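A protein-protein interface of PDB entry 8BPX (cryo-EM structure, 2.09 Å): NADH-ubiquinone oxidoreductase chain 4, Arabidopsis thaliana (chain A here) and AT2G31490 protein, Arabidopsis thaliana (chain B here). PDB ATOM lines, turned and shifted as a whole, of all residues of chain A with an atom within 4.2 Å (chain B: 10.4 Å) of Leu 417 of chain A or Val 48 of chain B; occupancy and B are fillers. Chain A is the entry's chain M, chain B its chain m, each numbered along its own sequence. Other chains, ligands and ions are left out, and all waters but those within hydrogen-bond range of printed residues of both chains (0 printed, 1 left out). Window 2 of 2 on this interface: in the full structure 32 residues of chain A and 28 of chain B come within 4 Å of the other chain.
Of the 18 printed residues of chain B, 5 touch a printed residue of chain A.
Printed residues of chain B that touch a printed residue of chain A: Pro 45, Val 48, Tyr 49, Gly 51 and Ile 52.
Of the 10 printed residues of chain A, 4 touch a printed residue of chain B.
Printed residues of chain A that touch a printed residue of chain B: Thr 285, Leu 413, Val 414 and Leu 417.
Hydrophobic or aromatic side chains of chain A that line the printed part of chain B: Leu 413, Val 414 and Leu 417.
Along chain A the printed residues that touch a printed residue of chain B span positions 285 to 417.
Among the printed residues, no Asp or Glu carboxylate lies within 4 Å of a Lys or Arg side-chain nitrogen of the other chain.
Thr 285 of chain A touches Pro 45 of chain B (CG2 to O, 3.4 Å).
Val 48 of chain B touches Thr 285 of chain A (CG1 to CG2, 3.9 Å).
Thr 285 of chain A touches Tyr 49 of chain B (OG1 to CA, 3.3 Å).
OG1 of Thr 285 of chain A touches CD1 of Ile 52 of chain B, at 3.5 Å.
Leu 413 of chain A touches Gly 51 of chain B (CD2 to C, 3.7 Å).
Leu 413 of chain A touches Ile 52 of chain B.
CG1 of Ile 52 of chain B touches CG1 of Val 414 of chain A, 3.5 Å away.
CD1 of Leu 417 of chain A touches CG1 of Val 48 of chain B (3.9 Å).
Of chain B, only Pro 45, Val 48, Tyr 49 and Ile 52 come within 4 Å of Thr 285 of chain A.
Ile 292 of chain A touches none of the printed residues of chain B.
Of the printed residues of chain B, Val 414 of chain A touches Ile 52 (3.5 Å).
Ala 415 of chain A touches none of the printed residues of chain B.
No residue of chain B comes within 4 Å of Thr 416 of chain A.
Of chain B, only Val 48 comes within 4 Å of Leu 417 of chain A.
Ala 418 of chain A touches none of the printed residues of chain B.
Ala 419 of chain A touches none of the printed residues of chain B.
No residue of chain B comes within 4 Å of Leu 420 of chain A.
Ile 42 of chain B touches none of the printed residues of chain A.
Val 48 of chain B touches just these residues of chain A: Thr 285 (3.9 Å) and Leu 417 (3.9 Å).
Printed residues of chain A within 4 Å of Gly 51 of chain B: Leu 413 (3.7 Å).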
ATOM      1  N   THR A 285     -14.913 -23.005 -29.324  1.00  0.00           N
ATOM      2  CA  THR A 285     -13.608 -22.393 -29.548  1.00  0.00           C
ATOM      3  C   THR A 285     -13.686 -20.873 -29.456  1.00  0.00           C
ATOM      4  O   THR A 285     -12.885 -20.241 -28.753  1.00  0.00           O
ATOM      5  CB  THR A 285     -13.054 -22.822 -30.909  1.00  0.00           C
ATOM      6  OG1 THR A 285     -13.104 -24.246 -31.022  1.00  0.00           O
ATOM      7  CG2 THR A 285     -11.624 -22.357 -31.077  1.00  0.00           C
ATOM      8  N   ILE A 292     -10.610 -16.115 -22.240  1.00  0.00           N
ATOM      9  CA  ILE A 292      -9.170 -15.926 -21.919  1.00  0.00           C
ATOM     10  C   ILE A 292      -8.617 -14.574 -22.428  1.00  0.00           C
ATOM     11  O   ILE A 292      -8.156 -13.831 -21.597  1.00  0.00           O
ATOM     12  CB  ILE A 292      -8.259 -17.072 -22.447  1.00  0.00           C
ATOM     13  CG1 ILE A 292      -8.704 -18.454 -21.955  1.00  0.00           C
ATOM     14  CG2 ILE A 292      -6.801 -16.810 -22.143  1.00  0.00           C
ATOM     15  CD1 ILE A 292      -9.100 -18.486 -20.518  1.00  0.00           C
ATOM     16  N   LEU A 413     -12.507 -30.465 -21.971  1.00  0.00           N
ATOM     17  CA  LEU A 413     -11.577 -29.371 -22.345  1.00  0.00           C
ATOM     18  C   LEU A 413     -12.230 -27.964 -22.331  1.00  0.00           C
ATOM     19  O   LEU A 413     -11.622 -27.058 -21.783  1.00  0.00           O
ATOM     20  CB  LEU A 413     -10.893 -29.674 -23.686  1.00  0.00           C
ATOM     21  CG  LEU A 413      -9.897 -28.640 -24.191  1.00  0.00           C
ATOM     22  CD1 LEU A 413      -8.744 -28.457 -23.221  1.00  0.00           C
ATOM     23  CD2 LEU A 413      -9.398 -29.002 -25.577  1.00  0.00           C
ATOM     24  N   VAL A 414     -13.388 -27.834 -22.934  1.00  0.00           N
ATOM     25  CA  VAL A 414     -14.086 -26.524 -22.965  1.00  0.00           C
ATOM     26  C   VAL A 414     -14.439 -26.072 -21.531  1.00  0.00           C
ATOM     27  O   VAL A 414     -14.179 -24.945 -21.199  1.00  0.00           O
ATOM     28  CB  VAL A 414     -15.255 -26.503 -23.994  1.00  0.00           C
ATOM     29  CG1 VAL A 414     -14.913 -27.264 -25.251  1.00  0.00           C
ATOM     30  CG2 VAL A 414     -16.596 -26.941 -23.435  1.00  0.00           C
ATOM     31  N   ALA A 415     -14.895 -26.991 -20.690  1.00  0.00           N
ATOM     32  CA  ALA A 415     -15.160 -26.673 -19.268  1.00  0.00           C
ATOM     33  C   ALA A 415     -13.869 -26.211 -18.576  1.00  0.00           C
ATOM     34  O   ALA A 415     -13.937 -25.270 -17.844  1.00  0.00           O
ATOM     35  CB  ALA A 415     -15.856 -27.813 -18.586  1.00  0.00           C
ATOM     36  N   THR A 416     -12.760 -26.837 -18.904  1.00  0.00           N
ATOM     37  CA  THR A 416     -11.456 -26.522 -18.279  1.00  0.00           C
ATOM     38  C   THR A 416     -10.999 -25.106 -18.702  1.00  0.00           C
ATOM     39  O   THR A 416     -10.608 -24.346 -17.851  1.00  0.00           O
ATOM     40  CB  THR A 416     -10.475 -27.682 -18.525  1.00  0.00           C
ATOM     41  OG1 THR A 416     -10.886 -28.836 -17.797  1.00  0.00           O
ATOM     42  CG2 THR A 416      -9.056 -27.330 -18.139  1.00  0.00           C
ATOM     43  N   LEU A 417     -11.127 -24.792 -19.979  1.00  0.00           N
ATOM     44  CA  LEU A 417     -10.772 -23.448 -20.493  1.00  0.00           C
ATOM     45  C   LEU A 417     -11.733 -22.408 -19.887  1.00  0.00           C
ATOM     46  O   LEU A 417     -11.239 -21.401 -19.451  1.00  0.00           O
ATOM     47  CB  LEU A 417     -10.782 -23.530 -22.016  1.00  0.00           C
ATOM     48  CG  LEU A 417      -9.772 -24.412 -22.748  1.00  0.00           C
ATOM     49  CD1 LEU A 417      -9.991 -24.504 -24.243  1.00  0.00           C
ATOM     50  CD2 LEU A 417      -8.356 -24.002 -22.406  1.00  0.00           C
ATOM     51  N   ALA A 418     -13.015 -22.697 -19.789  1.00  0.00           N
ATOM     52  CA  ALA A 418     -14.041 -21.803 -19.195  1.00  0.00           C
ATOM     53  C   ALA A 418     -13.867 -21.601 -17.680  1.00  0.00           C
ATOM     54  O   ALA A 418     -14.052 -20.514 -17.256  1.00  0.00           O
ATOM     55  CB  ALA A 418     -15.417 -22.243 -19.573  1.00  0.00           C
ATOM     56  N   ALA A 419     -13.396 -22.602 -16.950  1.00  0.00           N
ATOM     57  CA  ALA A 419     -13.136 -22.447 -15.510  1.00  0.00           C
ATOM     58  C   ALA A 419     -11.904 -21.516 -15.236  1.00  0.00           C
ATOM     59  O   ALA A 419     -11.840 -21.042 -14.159  1.00  0.00           O
ATOM     60  CB  ALA A 419     -13.086 -23.796 -14.861  1.00  0.00           C
ATOM     61  N   LEU A 420     -10.984 -21.318 -16.190  1.00  0.00           N
ATOM     62  CA  LEU A 420      -9.882 -20.290 -16.074  1.00  0.00           C
ATOM     63  C   LEU A 420     -10.438 -18.898 -15.760  1.00  0.00           C
ATOM     64  O   LEU A 420      -9.761 -18.192 -15.047  1.00  0.00           O
ATOM     65  CB  LEU A 420      -9.000 -20.244 -17.321  1.00  0.00           C
ATOM     66  CG  LEU A 420      -8.197 -21.518 -17.566  1.00  0.00           C
ATOM     67  CD1 LEU A 420      -7.501 -21.487 -18.915  1.00  0.00           C
ATOM     68  CD2 LEU A 420      -7.216 -21.777 -16.438  1.00  0.00           C
ATOM     69  N   ILE B  39       0.546 -16.260 -34.425  1.00  0.00           N
ATOM     70  CA  ILE B  39       0.557 -17.252 -33.358  1.00  0.00           C
ATOM     71  C   ILE B  39      -0.757 -17.233 -32.588  1.00  0.00           C
ATOM     72  O   ILE B  39      -1.416 -18.266 -32.430  1.00  0.00           O
ATOM     73  CB  ILE B  39       1.759 -17.019 -32.428  1.00  0.00           C
ATOM     74  CG1 ILE B  39       3.062 -17.383 -33.141  1.00  0.00           C
ATOM     75  CG2 ILE B  39       1.602 -17.822 -31.137  1.00  0.00           C
ATOM     76  CD1 ILE B  39       4.260 -16.620 -32.645  1.00  0.00           C
ATOM     77  N   PHE B  40      -1.176 -16.042 -32.175  1.00  0.00           N
ATOM     78  CA  PHE B  40      -2.317 -15.902 -31.241  1.00  0.00           C
ATOM     79  C   PHE B  40      -3.635 -15.641 -31.949  1.00  0.00           C
ATOM     80  O   PHE B  40      -4.634 -15.916 -31.425  1.00  0.00           O
ATOM     81  CB  PHE B  40      -1.936 -14.888 -30.175  1.00  0.00           C
ATOM     82  CG  PHE B  40      -0.816 -15.370 -29.293  1.00  0.00           C
ATOM     83  CD1 PHE B  40      -1.008 -16.454 -28.449  1.00  0.00           C
ATOM     84  CD2 PHE B  40       0.425 -14.758 -29.310  1.00  0.00           C
ATOM     85  CE1 PHE B  40       0.017 -16.907 -27.633  1.00  0.00           C
ATOM     86  CE2 PHE B  40       1.449 -15.213 -28.496  1.00  0.00           C
ATOM     87  CZ  PHE B  40       1.243 -16.284 -27.655  1.00  0.00           C
ATOM     88  N   GLY B  41      -3.609 -15.221 -33.212  1.00  0.00           N
ATOM     89  CA  GLY B  41      -4.855 -14.915 -33.942  1.00  0.00           C
ATOM     90  C   GLY B  41      -5.318 -15.998 -34.896  1.00  0.00           C
ATOM     91  O   GLY B  41      -6.512 -16.024 -35.179  1.00  0.00           O
ATOM     92  N   ILE B  42      -4.402 -16.845 -35.384  1.00  0.00           N
ATOM     93  CA  ILE B  42      -4.703 -18.009 -36.270  1.00  0.00           C
ATOM     94  C   ILE B  42      -4.342 -19.290 -35.508  1.00  0.00           C
ATOM     95  O   ILE B  42      -5.265 -20.062 -35.231  1.00  0.00           O
ATOM     96  CB  ILE B  42      -3.989 -17.883 -37.644  1.00  0.00           C
ATOM     97  CG1 ILE B  42      -4.639 -16.803 -38.511  1.00  0.00           C
ATOM     98  CG2 ILE B  42      -3.916 -19.211 -38.373  1.00  0.00           C
ATOM     99  CD1 ILE B  42      -3.930 -15.476 -38.481  1.00  0.00           C
ATOM    100  N   ALA B  43      -3.064 -19.483 -35.163  1.00  0.00           N
ATOM    101  CA  ALA B  43      -2.601 -20.818 -34.789  1.00  0.00           C
ATOM    102  C   ALA B  43      -3.280 -21.322 -33.519  1.00  0.00           C
ATOM    103  O   ALA B  43      -3.840 -22.423 -33.500  1.00  0.00           O
ATOM    104  CB  ALA B  43      -1.081 -20.823 -34.625  1.00  0.00           C
ATOM    105  N   LEU B  44      -3.247 -20.526 -32.448  1.00  0.00           N
ATOM    106  CA  LEU B  44      -3.823 -20.971 -31.179  1.00  0.00           C
ATOM    107  C   LEU B  44      -5.315 -21.272 -31.272  1.00  0.00           C
ATOM    108  O   LEU B  44      -5.741 -22.317 -30.751  1.00  0.00           O
ATOM    109  CB  LEU B  44      -3.525 -19.942 -30.083  1.00  0.00           C
ATOM    110  CG  LEU B  44      -3.823 -20.378 -28.647  1.00  0.00           C
ATOM    111  CD1 LEU B  44      -3.396 -21.824 -28.412  1.00  0.00           C
ATOM    112  CD2 LEU B  44      -3.168 -19.450 -27.638  1.00  0.00           C
ATOM    113  N   PRO B  45      -6.157 -20.429 -31.885  1.00  0.00           N
ATOM    114  CA  PRO B  45      -7.560 -20.836 -32.078  1.00  0.00           C
ATOM    115  C   PRO B  45      -7.716 -22.129 -32.860  1.00  0.00           C
ATOM    116  O   PRO B  45      -8.591 -22.936 -32.532  1.00  0.00           O
ATOM    117  CB  PRO B  45      -8.164 -19.642 -32.826  1.00  0.00           C
ATOM    118  CG  PRO B  45      -7.317 -18.500 -32.439  1.00  0.00           C
ATOM    119  CD  PRO B  45      -5.938 -19.039 -32.323  1.00  0.00           C
ATOM    120  N   ILE B  46      -6.885 -22.356 -33.880  1.00  0.00           N
ATOM    121  CA  ILE B  46      -6.956 -23.602 -34.638  1.00  0.00           C
ATOM    122  C   ILE B  46      -6.600 -24.787 -33.749  1.00  0.00           C
ATOM    123  O   ILE B  46      -7.246 -25.839 -33.800  1.00  0.00           O
ATOM    124  CB  ILE B  46      -6.047 -23.531 -35.879  1.00  0.00           C
ATOM    125  CG1 ILE B  46      -6.634 -22.586 -36.927  1.00  0.00           C
ATOM    126  CG2 ILE B  46      -5.849 -24.908 -36.487  1.00  0.00           C
ATOM    127  CD1 ILE B  46      -5.698 -22.310 -38.073  1.00  0.00           C
ATOM    128  N   ILE B  47      -5.565 -24.630 -32.923  1.00  0.00           N
ATOM    129  CA  ILE B  47      -5.150 -25.693 -32.016  1.00  0.00           C
ATOM    130  C   ILE B  47      -6.258 -26.006 -31.015  1.00  0.00           C
ATOM    131  O   ILE B  47      -6.558 -27.174 -30.745  1.00  0.00           O
ATOM    132  CB  ILE B  47      -3.834 -25.303 -31.319  1.00  0.00           C
ATOM    133  CG1 ILE B  47      -2.665 -25.399 -32.303  1.00  0.00           C
ATOM    134  CG2 ILE B  47      -3.581 -26.167 -30.096  1.00  0.00           C
ATOM    135  CD1 ILE B  47      -1.438 -24.657 -31.868  1.00  0.00           C
ATOM    136  N   VAL B  48      -6.899 -24.970 -30.469  1.00  0.00           N
ATOM    137  CA  VAL B  48      -7.999 -25.183 -29.529  1.00  0.00           C
ATOM    138  C   VAL B  48      -9.170 -25.878 -30.213  1.00  0.00           C
ATOM    139  O   VAL B  48      -9.793 -26.782 -29.640  1.00  0.00           O
ATOM    140  CB  VAL B  48      -8.423 -23.845 -28.893  1.00  0.00           C
ATOM    141  CG1 VAL B  48      -9.727 -24.003 -28.140  1.00  0.00           C
ATOM    142  CG2 VAL B  48      -7.337 -23.346 -27.959  1.00  0.00           C
ATOM    143  N   TYR B  49      -9.497 -25.463 -31.442  1.00  0.00           N
ATOM    144  CA  TYR B  49     -10.581 -26.108 -32.174  1.00  0.00           C
ATOM    145  C   TYR B  49     -10.285 -27.584 -32.411  1.00  0.00           C
ATOM    146  O   TYR B  49     -11.161 -28.438 -32.225  1.00  0.00           O
ATOM    147  CB  TYR B  49     -10.819 -25.388 -33.503  1.00  0.00           C
ATOM    148  CG  TYR B  49     -11.887 -26.026 -34.357  1.00  0.00           C
ATOM    149  CD1 TYR B  49     -11.567 -26.986 -35.310  1.00  0.00           C
ATOM    150  CD2 TYR B  49     -13.219 -25.666 -34.212  1.00  0.00           C
ATOM    151  CE1 TYR B  49     -12.547 -27.573 -36.087  1.00  0.00           C
ATOM    152  CE2 TYR B  49     -14.203 -26.245 -34.984  1.00  0.00           C
ATOM    153  CZ  TYR B  49     -13.860 -27.198 -35.920  1.00  0.00           C
ATOM    154  OH  TYR B  49     -14.838 -27.771 -36.688  1.00  0.00           O
ATOM    155  N   LYS B  50      -9.089 -27.900 -32.848  1.00  0.00           N
ATOM    156  CA  LYS B  50      -8.637 -29.316 -33.080  1.00  0.00           C
ATOM    157  C   LYS B  50      -8.701 -30.107 -31.756  1.00  0.00           C
ATOM    158  O   LYS B  50      -9.246 -31.173 -31.802  1.00  0.00           O
ATOM    159  CB  LYS B  50      -7.340 -29.341 -33.899  1.00  0.00           C
ATOM    160  CG  LYS B  50      -7.521 -28.950 -35.352  1.00  0.00           C
ATOM    161  CD  LYS B  50      -6.294 -29.191 -36.180  1.00  0.00           C
ATOM    162  CE  LYS B  50      -6.534 -28.849 -37.632  1.00  0.00           C
ATOM    163  NZ  LYS B  50      -7.681 -29.608 -38.182  1.00  0.00           N
ATOM    164  N   GLY B  51      -8.395 -29.488 -30.623  1.00  0.00           N
ATOM    165  CA  GLY B  51      -8.520 -30.115 -29.296  1.00  0.00           C
ATOM    166  C   GLY B  51      -9.942 -30.472 -28.933  1.00  0.00           C
ATOM    167  O   GLY B  51     -10.146 -31.600 -28.589  1.00  0.00           O
ATOM    168  N   ILE B  52     -10.879 -29.550 -29.130  1.00  0.00           N
ATOM    169  CA  ILE B  52     -12.303 -29.706 -28.801  1.00  0.00           C
ATOM    170  C   ILE B  52     -12.865 -30.817 -29.671  1.00  0.00           C
ATOM    171  O   ILE B  52     -13.567 -31.636 -29.111  1.00  0.00           O
ATOM    172  CB  ILE B  52     -13.044 -28.320 -28.856  1.00  0.00           C
ATOM    173  CG1 ILE B  52     -12.533 -27.343 -27.796  1.00  0.00           C
ATOM    174  CG2 ILE B  52     -14.557 -28.484 -28.821  1.00  0.00           C
ATOM    175  CD1 ILE B  52     -12.999 -25.926 -27.964  1.00  0.00           C
ATOM    176  N   VAL B  53     -12.511 -30.844 -30.950  1.00  0.00           N
ATOM    177  CA  VAL B  53     -13.059 -31.820 -31.917  1.00  0.00           C
ATOM    178  C   VAL B  53     -12.561 -33.227 -31.568  1.00  0.00           C
ATOM    179  O   VAL B  53     -13.344 -34.105 -31.547  1.00  0.00           O
ATOM    180  CB  VAL B  53     -12.840 -31.414 -33.403  1.00  0.00           C
ATOM    181  CG1 VAL B  53     -13.040 -32.557 -34.383  1.00  0.00           C
ATOM    182  CG2 VAL B  53     -13.632 -30.183 -33.809  1.00  0.00           C
ATOM    183  N   LYS B  54     -11.296 -33.333 -31.273  1.00  0.00           N
ATOM    184  CA  LYS B  54     -10.657 -34.599 -30.905  1.00  0.00           C
ATOM    185  C   LYS B  54     -11.325 -35.133 -29.628  1.00  0.00           C
ATOM    186  O   LYS B  54     -11.559 -36.300 -29.576  1.00  0.00           O
ATOM    187  CB  LYS B  54      -9.155 -34.371 -30.813  1.00  0.00           C
ATOM    188  CG  LYS B  54      -8.396 -35.384 -29.969  1.00  0.00           C
ATOM    189  CD  LYS B  54      -6.911 -35.333 -30.212  1.00  0.00           C
ATOM    190  CE  LYS B  54      -6.198 -36.610 -29.821  1.00  0.00           C
ATOM    191  NZ  LYS B  54      -6.032 -36.733 -28.355  1.00  0.00           N
ATOM    192  N   ASP B  55     -11.573 -34.263 -28.688  1.00  0.00           N
ATOM    193  CA  ASP B  55     -12.267 -34.634 -27.446  1.00  0.00           C
ATOM    194  C   ASP B  55     -13.588 -35.322 -27.814  1.00  0.00           C
ATOM    195  O   ASP B  55     -13.720 -36.487 -27.414  1.00  0.00           O
ATOM    196  CB  ASP B  55     -12.370 -33.402 -26.561  1.00  0.00           C
ATOM    197  CG  ASP B  55     -13.042 -33.628 -25.231  1.00  0.00           C
ATOM    198  OD1 ASP B  55     -12.483 -34.378 -24.420  1.00  0.00           O
ATOM    199  OD2 ASP B  55     -14.120 -33.067 -25.025  1.00  0.00           O
ATOM    200  N   PHE B  56     -14.419 -34.705 -28.662  1.00  0.00           N
ATOM    201  CA  PHE B  56     -15.651 -35.368 -29.121  1.00  0.00           C
ATOM    202  C   PHE B  56     -15.356 -36.718 -29.841  1.00  0.00           C
ATOM    203  O   PHE B  56     -16.165 -37.603 -29.681  1.00  0.00           O
ATOM    204  CB  PHE B  56     -16.545 -34.466 -29.983  1.00  0.00           C
ATOM    205  CG  PHE B  56     -17.226 -33.293 -29.316  1.00  0.00           C
ATOM    206  CD1 PHE B  56     -18.203 -33.481 -28.349  1.00  0.00           C
ATOM    207  CD2 PHE B  56     -16.954 -31.996 -29.716  1.00  0.00           C
ATOM    208  CE1 PHE B  56     -18.863 -32.406 -27.778  1.00  0.00           C
ATOM    209  CE2 PHE B  56     -17.608 -30.915 -29.141  1.00  0.00           C
ATOM    210  CZ  PHE B  56     -18.569 -31.119 -28.179  1.00  0.00           C
